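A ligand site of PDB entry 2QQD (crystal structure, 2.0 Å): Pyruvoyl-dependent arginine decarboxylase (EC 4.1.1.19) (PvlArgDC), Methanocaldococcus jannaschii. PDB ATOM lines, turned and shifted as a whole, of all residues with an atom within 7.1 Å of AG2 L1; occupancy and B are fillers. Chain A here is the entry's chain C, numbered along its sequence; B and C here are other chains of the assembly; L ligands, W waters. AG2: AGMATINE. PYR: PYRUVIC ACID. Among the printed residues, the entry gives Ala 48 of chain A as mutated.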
ATOM      1  N   PRO A  31      13.899  -9.911  18.953  1.00  0.00           N
ATOM      2  CA  PRO A  31      15.291  -9.476  19.027  1.00  0.00           C
ATOM      3  C   PRO A  31      15.475  -8.079  18.427  1.00  0.00           C
ATOM      4  O   PRO A  31      16.174  -7.244  18.993  1.00  0.00           O
ATOM      5  CB  PRO A  31      16.024 -10.552  18.237  1.00  0.00           C
ATOM      6  CG  PRO A  31      15.186 -11.781  18.493  1.00  0.00           C
ATOM      7  CD  PRO A  31      13.789 -11.241  18.324  1.00  0.00           C
ATOM      8  N   LEU A  32      14.852  -7.840  17.278  1.00  0.00           N
ATOM      9  CA  LEU A  32      14.998  -6.551  16.638  1.00  0.00           C
ATOM     10  C   LEU A  32      14.363  -5.439  17.470  1.00  0.00           C
ATOM     11  O   LEU A  32      14.881  -4.309  17.501  1.00  0.00           O
ATOM     12  CB  LEU A  32      14.415  -6.585  15.232  1.00  0.00           C
ATOM     13  CG  LEU A  32      14.805  -5.413  14.329  1.00  0.00           C
ATOM     14  CD1 LEU A  32      16.328  -5.211  14.343  1.00  0.00           C
ATOM     15  CD2 LEU A  32      14.323  -5.702  12.910  1.00  0.00           C
ATOM     16  N   ASN A  33      13.260  -5.738  18.141  1.00  0.00           N
ATOM     17  CA  ASN A  33      12.602  -4.742  18.973  1.00  0.00           C
ATOM     18  C   ASN A  33      13.430  -4.451  20.226  1.00  0.00           C
ATOM     19  O   ASN A  33      13.423  -3.334  20.736  1.00  0.00           O
ATOM     20  CB  ASN A  33      11.184  -5.173  19.361  1.00  0.00           C
ATOM     21  CG  ASN A  33      10.200  -5.089  18.197  1.00  0.00           C
ATOM     22  OD1 ASN A  33       9.627  -6.102  17.771  1.00  0.00           O
ATOM     23  ND2 ASN A  33      10.015  -3.881  17.657  1.00  0.00           N
ATOM     24  N   PHE A  35      16.800  -4.760  20.379  1.00  0.00           N
ATOM     25  CA  PHE A  35      17.946  -4.019  19.867  1.00  0.00           C
ATOM     26  C   PHE A  35      17.521  -2.554  19.733  1.00  0.00           C
ATOM     27  O   PHE A  35      18.241  -1.640  20.145  1.00  0.00           O
ATOM     28  CB  PHE A  35      18.364  -4.583  18.502  1.00  0.00           C
ATOM     29  CG  PHE A  35      19.495  -3.845  17.835  1.00  0.00           C
ATOM     30  CD1 PHE A  35      20.813  -4.059  18.219  1.00  0.00           C
ATOM     31  CD2 PHE A  35      19.236  -2.973  16.776  1.00  0.00           C
ATOM     32  CE1 PHE A  35      21.867  -3.405  17.560  1.00  0.00           C
ATOM     33  CE2 PHE A  35      20.271  -2.331  16.108  1.00  0.00           C
ATOM     34  CZ  PHE A  35      21.593  -2.542  16.501  1.00  0.00           C
ATOM     35  N   ASP A  36      16.347  -2.340  19.140  1.00  0.00           N
ATOM     36  CA  ASP A  36      15.797  -0.994  18.934  1.00  0.00           C
ATOM     37  C   ASP A  36      15.609  -0.316  20.280  1.00  0.00           C
ATOM     38  O   ASP A  36      15.919   0.859  20.447  1.00  0.00           O
ATOM     39  CB  ASP A  36      14.458  -1.064  18.188  1.00  0.00           C
ATOM     40  CG  ASP A  36      13.928   0.303  17.787  1.00  0.00           C
ATOM     41  OD1 ASP A  36      14.738   1.145  17.346  1.00  0.00           O
ATOM     42  OD2 ASP A  36      12.707   0.550  17.895  1.00  0.00           O
ATOM     43  N   GLY A  37      15.087  -1.071  21.245  1.00  0.00           N
ATOM     44  CA  GLY A  37      14.877  -0.507  22.567  1.00  0.00           C
ATOM     45  C   GLY A  37      16.202  -0.122  23.201  1.00  0.00           C
ATOM     46  O   GLY A  37      16.293   0.871  23.932  1.00  0.00           O
ATOM     47  N   LEU A  39      18.991   0.789  21.539  1.00  0.00           N
ATOM     48  CA  LEU A  39      19.500   1.984  20.882  1.00  0.00           C
ATOM     49  C   LEU A  39      18.762   3.210  21.441  1.00  0.00           C
ATOM     50  O   LEU A  39      19.391   4.221  21.766  1.00  0.00           O
ATOM     51  CB  LEU A  39      19.313   1.889  19.361  1.00  0.00           C
ATOM     52  CG  LEU A  39      20.495   1.269  18.587  1.00  0.00           C
ATOM     53  CD1 LEU A  39      20.832  -0.118  19.100  1.00  0.00           C
ATOM     54  CD2 LEU A  39      20.136   1.203  17.116  1.00  0.00           C
ATOM     55  N   LEU A  40      17.443   3.089  21.597  1.00  0.00           N
ATOM     56  CA  LEU A  40      16.615   4.155  22.159  1.00  0.00           C
ATOM     57  C   LEU A  40      17.103   4.533  23.558  1.00  0.00           C
ATOM     58  O   LEU A  40      17.197   5.714  23.900  1.00  0.00           O
ATOM     59  CB  LEU A  40      15.151   3.708  22.258  1.00  0.00           C
ATOM     60  CG  LEU A  40      14.292   3.726  20.987  1.00  0.00           C
ATOM     61  CD1 LEU A  40      13.055   2.882  21.191  1.00  0.00           C
ATOM     62  CD2 LEU A  40      13.923   5.167  20.664  1.00  0.00           C
ATOM     63  N   ILE A  44      20.457   6.964  20.803  1.00  0.00           N
ATOM     64  CA  ILE A  44      20.585   7.025  19.345  1.00  0.00           C
ATOM     65  C   ILE A  44      19.541   6.141  18.676  1.00  0.00           C
ATOM     66  O   ILE A  44      19.825   5.502  17.667  1.00  0.00           O
ATOM     67  CB  ILE A  44      21.983   6.573  18.862  1.00  0.00           C
ATOM     68  CG1 ILE A  44      22.332   5.192  19.425  1.00  0.00           C
ATOM     69  CG2 ILE A  44      23.024   7.610  19.249  1.00  0.00           C
ATOM     70  CD1 ILE A  44      23.708   4.672  19.010  1.00  0.00           C
ATOM     71  N   GLY A  45      18.341   6.113  19.234  1.00  0.00           N
ATOM     72  CA  GLY A  45      17.296   5.282  18.679  1.00  0.00           C
ATOM     73  C   GLY A  45      16.622   5.837  17.438  1.00  0.00           C
ATOM     74  O   GLY A  45      16.032   5.080  16.659  1.00  0.00           O
ATOM     75  N   ASN A  46      16.751   7.139  17.228  1.00  0.00           N
ATOM     76  CA  ASN A  46      16.100   7.763  16.094  1.00  0.00           C
ATOM     77  C   ASN A  46      16.988   8.256  14.950  1.00  0.00           C
ATOM     78  O   ASN A  46      16.710   9.273  14.330  1.00  0.00           O
ATOM     79  CB  ASN A  46      15.182   8.867  16.611  1.00  0.00           C
ATOM     80  CG  ASN A  46      14.100   8.326  17.533  1.00  0.00           C
ATOM     81  OD1 ASN A  46      13.405   7.367  17.180  1.00  0.00           O
ATOM     82  ND2 ASN A  46      13.955   8.913  18.707  1.00  0.00           N
ATOM     83  N   VAL A  47      18.064   7.520  14.694  1.00  0.00           N
ATOM     84  CA  VAL A  47      18.968   7.812  13.591  1.00  0.00           C
ATOM     85  C   VAL A  47      19.290   6.447  12.984  1.00  0.00           C
ATOM     86  O   VAL A  47      19.124   5.413  13.640  1.00  0.00           O
ATOM     87  CB  VAL A  47      20.315   8.472  14.022  1.00  0.00           C
ATOM     88  CG1 VAL A  47      20.047   9.808  14.714  1.00  0.00           C
ATOM     89  CG2 VAL A  47      21.102   7.541  14.927  1.00  0.00           C
ATOM     90  N   ALA A  48      19.738   6.444  11.749  1.00  0.00           N
ATOM     91  CA  ALA A  48      20.085   5.208  11.089  1.00  0.00           C
ATOM     92  C   ALA A  48      21.573   4.999  11.343  1.00  0.00           C
ATOM     93  O   ALA A  48      22.377   5.910  11.143  1.00  0.00           O
ATOM     94  CB  ALA A  48      19.818   5.312   9.586  1.00  0.00           C
ATOM     95  N   LEU A  49      21.924   3.808  11.811  1.00  0.00           N
ATOM     96  CA  LEU A  49      23.316   3.512  12.086  1.00  0.00           C
ATOM     97  C   LEU A  49      24.001   2.843  10.902  1.00  0.00           C
ATOM     98  O   LEU A  49      23.444   1.932  10.294  1.00  0.00           O
ATOM     99  CB  LEU A  49      23.453   2.588  13.309  1.00  0.00           C
ATOM    100  CG  LEU A  49      22.919   3.044  14.665  1.00  0.00           C
ATOM    101  CD1 LEU A  49      23.354   2.024  15.731  1.00  0.00           C
ATOM    102  CD2 LEU A  49      23.444   4.433  15.014  1.00  0.00           C
ATOM    103  N   ILE B   1      15.786   3.668  10.170  1.00  0.00           N
ATOM    104  CA  ILE B   1      15.038   4.901  10.401  1.00  0.00           C
ATOM    105  C   ILE B   1      14.840   5.680   9.113  1.00  0.00           C
ATOM    106  O   ILE B   1      15.779   5.828   8.330  1.00  0.00           O
ATOM    107  CB  ILE B   1      15.781   5.812  11.415  1.00  0.00           C
ATOM    108  CG1 ILE B   1      15.806   5.155  12.795  1.00  0.00           C
ATOM    109  CG2 ILE B   1      15.129   7.183  11.468  1.00  0.00           C
ATOM    110  CD1 ILE B   1      14.458   5.076  13.484  1.00  0.00           C
ATOM    111  N   ALA B  23      17.904  -0.498   4.236  1.00  0.00           N
ATOM    112  CA  ALA B  23      17.565  -1.353   5.368  1.00  0.00           C
ATOM    113  C   ALA B  23      17.006  -2.590   4.695  1.00  0.00           C
ATOM    114  O   ALA B  23      16.107  -2.500   3.861  1.00  0.00           O
ATOM    115  CB  ALA B  23      16.497  -0.698   6.246  1.00  0.00           C
ATOM    116  N   ILE B  40       9.563  -6.301   4.826  1.00  0.00           N
ATOM    117  CA  ILE B  40       9.998  -4.992   5.308  1.00  0.00           C
ATOM    118  C   ILE B  40       8.773  -4.133   5.584  1.00  0.00           C
ATOM    119  O   ILE B  40       7.777  -4.194   4.861  1.00  0.00           O
ATOM    120  CB  ILE B  40      10.867  -4.262   4.244  1.00  0.00           C
ATOM    121  CG1 ILE B  40      12.272  -4.848   4.210  1.00  0.00           C
ATOM    122  CG2 ILE B  40      10.954  -2.766   4.564  1.00  0.00           C
ATOM    123  CD1 ILE B  40      13.122  -4.490   5.418  1.00  0.00           C
ATOM    124  N   SER B  41       8.836  -3.333   6.650  1.00  0.00           N
ATOM    125  CA  SER B  41       7.732  -2.459   7.009  1.00  0.00           C
ATOM    126  C   SER B  41       8.258  -1.061   7.355  1.00  0.00           C
ATOM    127  O   SER B  41       9.394  -0.924   7.813  1.00  0.00           O
ATOM    128  CB  SER B  41       6.952  -3.027   8.187  1.00  0.00           C
ATOM    129  OG  SER B  41       7.766  -3.103   9.347  1.00  0.00           O
ATOM    130  N   LEU B  53       9.916   4.538  11.257  1.00  0.00           N
ATOM    131  CA  LEU B  53      10.665   3.361  11.693  1.00  0.00           C
ATOM    132  C   LEU B  53      10.607   2.250  10.661  1.00  0.00           C
ATOM    133  O   LEU B  53       9.533   1.885  10.191  1.00  0.00           O
ATOM    134  CB  LEU B  53      10.106   2.860  13.037  1.00  0.00           C
ATOM    135  CG  LEU B  53      10.667   1.562  13.636  1.00  0.00           C
ATOM    136  CD1 LEU B  53      12.143   1.730  13.970  1.00  0.00           C
ATOM    137  CD2 LEU B  53       9.874   1.209  14.897  1.00  0.00           C
ATOM    138  N   ILE B  54      11.768   1.717  10.284  1.00  0.00           N
ATOM    139  CA  ILE B  54      11.846   0.633   9.311  1.00  0.00           C
ATOM    140  C   ILE B  54      12.167  -0.656  10.051  1.00  0.00           C
ATOM    141  O   ILE B  54      13.117  -0.711  10.823  1.00  0.00           O
ATOM    142  CB  ILE B  54      12.975   0.863   8.293  1.00  0.00           C
ATOM    143  CG1 ILE B  54      12.762   2.180   7.546  1.00  0.00           C
ATOM    144  CG2 ILE B  54      13.036  -0.299   7.307  1.00  0.00           C
ATOM    145  CD1 ILE B  54      13.911   2.519   6.625  1.00  0.00           C
ATOM    146  N   MET B  55      11.362  -1.683   9.826  1.00  0.00           N
ATOM    147  CA  MET B  55      11.581  -2.975  10.469  1.00  0.00           C
ATOM    148  C   MET B  55      11.685  -4.046   9.395  1.00  0.00           C
ATOM    149  O   MET B  55      11.031  -3.976   8.362  1.00  0.00           O
ATOM    150  CB  MET B  55      10.424  -3.304  11.414  1.00  0.00           C
ATOM    151  CG  MET B  55      10.488  -2.625  12.788  1.00  0.00           C
ATOM    152  SD  MET B  55      11.770  -3.331  13.885  1.00  0.00           S
ATOM    153  CE  MET B  55      11.894  -2.044  15.122  1.00  0.00           C
ATOM    154  N   GLU B  56      12.543  -5.027   9.616  1.00  0.00           N
ATOM    155  CA  GLU B  56      12.692  -6.118   8.678  1.00  0.00           C
ATOM    156  C   GLU B  56      12.527  -7.440   9.398  1.00  0.00           C
ATOM    157  O   GLU B  56      12.730  -7.531  10.601  1.00  0.00           O
ATOM    158  CB  GLU B  56      14.059  -6.068   7.974  1.00  0.00           C
ATOM    159  CG  GLU B  56      15.253  -6.015   8.887  1.00  0.00           C
ATOM    160  CD  GLU B  56      15.476  -4.627   9.449  1.00  0.00           C
ATOM    161  OE1 GLU B  56      15.561  -3.656   8.656  1.00  0.00           O
ATOM    162  OE2 GLU B  56      15.571  -4.520  10.686  1.00  0.00           O
ATOM    163  N   MET B  73       6.039  -5.767  14.401  1.00  0.00           N
ATOM    164  CA  MET B  73       7.305  -5.274  14.962  1.00  0.00           C
ATOM    165  C   MET B  73       7.378  -3.751  14.833  1.00  0.00           C
ATOM    166  O   MET B  73       7.872  -3.060  15.720  1.00  0.00           O
ATOM    167  CB  MET B  73       8.497  -5.916  14.248  1.00  0.00           C
ATOM    168  CG  MET B  73       8.696  -7.392  14.592  1.00  0.00           C
ATOM    169  SD  MET B  73       9.766  -8.235  13.416  1.00  0.00           S
ATOM    170  CE  MET B  73      11.355  -7.512  13.837  1.00  0.00           C
ATOM    171  N   ARG B  81       8.161   4.082  21.561  1.00  0.00           N
ATOM    172  CA  ARG B  81       8.482   5.502  21.469  1.00  0.00           C
ATOM    173  C   ARG B  81       7.304   6.339  21.962  1.00  0.00           C
ATOM    174  O   ARG B  81       7.457   7.516  22.285  1.00  0.00           O
ATOM    175  CB  ARG B  81       8.786   5.878  20.020  1.00  0.00           C
ATOM    176  CG  ARG B  81      10.054   5.261  19.457  1.00  0.00           C
ATOM    177  CD  ARG B  81      10.327   5.685  18.009  1.00  0.00           C
ATOM    178  NE  ARG B  81      11.687   5.339  17.596  1.00  0.00           N
ATOM    179  CZ  ARG B  81      12.181   4.093  17.591  1.00  0.00           C
ATOM    180  NH1 ARG B  81      11.424   3.077  17.986  1.00  0.00           N
ATOM    181  NH2 ARG B  81      13.438   3.880  17.241  1.00  0.00           N
ATOM    182  N   ILE C  52      21.923  -0.308   6.537  1.00  0.00           N
ATOM    183  CA  ILE C  52      21.735   0.564   7.682  1.00  0.00           C
ATOM    184  C   ILE C  52      21.024  -0.242   8.766  1.00  0.00           C
ATOM    185  O   ILE C  52      20.260  -1.164   8.463  1.00  0.00           O
ATOM    186  CB  ILE C  52      20.922   1.831   7.348  1.00  0.00           C
ATOM    187  CG1 ILE C  52      19.544   1.467   6.809  1.00  0.00           C
ATOM    188  CG2 ILE C  52      21.677   2.678   6.333  1.00  0.00           C
ATOM    189  CD1 ILE C  52      18.677   2.700   6.455  1.00  0.00           C
ATOM    190  N   SER C  53      21.270   0.122  10.019  1.00  0.00           N
ATOM    191  CA  SER C  53      20.694  -0.599  11.145  1.00  0.00           C
ATOM    192  C   SER C  53      20.144   0.260  12.279  1.00  0.00           C
ATOM    193  O   SER C  53      19.526  -0.327  13.175  1.00  0.00           O
ATOM    194  CB  SER C  53      21.743  -1.581  11.687  1.00  0.00           C
ATOM    195  OG  SER C  53      23.026  -0.970  11.707  1.00  0.00           O
ATOM    196  OXT SER C  53      20.347   1.491  12.275  1.00  0.00           O
HETATM  197  N   AG2 L   1      14.959  -2.078  11.605  1.00  0.00           N
HETATM  198  CA  AG2 L   1      15.998  -2.204  12.645  1.00  0.00           C
HETATM  199  CB  AG2 L   1      15.591  -1.496  13.913  1.00  0.00           C
HETATM  200  CG  AG2 L   1      16.632  -1.607  14.995  1.00  0.00           C
HETATM  201  CD  AG2 L   1      16.911  -0.289  15.678  1.00  0.00           C
HETATM  202  NE  AG2 L   1      17.527   0.699  14.790  1.00  0.00           N
HETATM  203  CZ  AG2 L   1      17.400   2.024  14.926  1.00  0.00           C
HETATM  204  NH1 AG2 L   1      16.664   2.535  15.902  1.00  0.00           N
HETATM  205  NH2 AG2 L   1      18.007   2.829  14.063  1.00  0.00           N
HETATM  206  C   PYR L   2      15.351   2.487  10.604  1.00  0.00           C
HETATM  207  O   PYR L   2      14.294   2.338  11.204  1.00  0.00           O
HETATM  208  CA  PYR L   2      16.190   1.374  10.322  1.00  0.00           C
HETATM  209  O3  PYR L   2      15.802   0.276  10.706  1.00  0.00           O
HETATM  210  CB  PYR L   2      17.512   1.345   9.596  1.00  0.00           C
HETATM  211  O   HOH W   1      18.957  -3.105  12.603  1.00  0.00           O
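The side-chain carboxylate (OD1) of Asp 36 lies within salt-bridge range of a nitrogen (NH1) of AG2 L1, 2.8 Å away. The backbone carbonyl oxygen (O) of Gly 45 sits at hydrogen-bond distance from a nitrogen (NH1) of AG2 L1, at 2.7 Å. The backbone carbonyl oxygen (O) of Val 47 is in hydrogen-bond range of a nitrogen (NH2) of AG2 L1, at 2.8 Å. The backbone NH (N) of Ile 54 of chain B lies within hydrogen-bond range of an oxygen (O) of PYR L2, 2.8 Å away. The chain-end carboxylate (O) of Ser 53 of chain C is in salt-bridge range of a nitrogen (NE) of AG2 L1. A carbon (C) of PYR L2 is bonded to the backbone NH (N) of Ile 1 of chain B, 1.3 Å away. N of AG2 L1 lies within hydrogen-bond range of O of Ile 54 of chain B (2.4 Å). A nitrogen (N) of AG2 L1 lies within salt-bridge range of the side-chain carboxylate (OE2) of Glu 56 of chain B, 2.7 Å away.
An oxygen (O3) of PYR L2 is in hydrogen-bond range of a nitrogen (N) of AG2 L1 (2.7 Å).
The side-chain carboxylate (OD2) of Asp 36 lies within salt-bridge range of the guanidinium group (NH1) of Arg 81 of chain B (2.8 Å). O of Met 55 of chain B lies within hydrogen-bond range of N of Ser 41 of chain B (2.9 Å). O of Gly 45 lies within hydrogen-bond range of NH2 of Arg 81 of chain B. OD1 of Asn 46 lies within hydrogen-bond range of NE of Arg 81 of chain B (2.7 Å). The chain-end carboxylate (OXT) of Ser 53 of chain C is in hydrogen-bond range of the backbone NH (N) of Leu 49, 2.8 Å away. N of Gly 45 lies within hydrogen-bond range of O of Leu 39 (3.3 Å). The backbone NH (N) of Ile 44 sits at hydrogen-bond distance from the backbone carbonyl oxygen (O) of Leu 39, 3.1 Å away.
Residues that only touch AG2 L1: Phe 35, Ile 1 of chain B, Leu 32, Leu 39, Met 55 of chain B and Arg 81 of chain B. Hydrophobic or aromatic side chains within 4 Å of AG2 L1: Leu 32, Phe 35, Leu 39, Ile 1 of chain B and Met 55 of chain B. The nearest printed residue that does not touch AG2 L1 is Ala 48 (4.3 Å).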
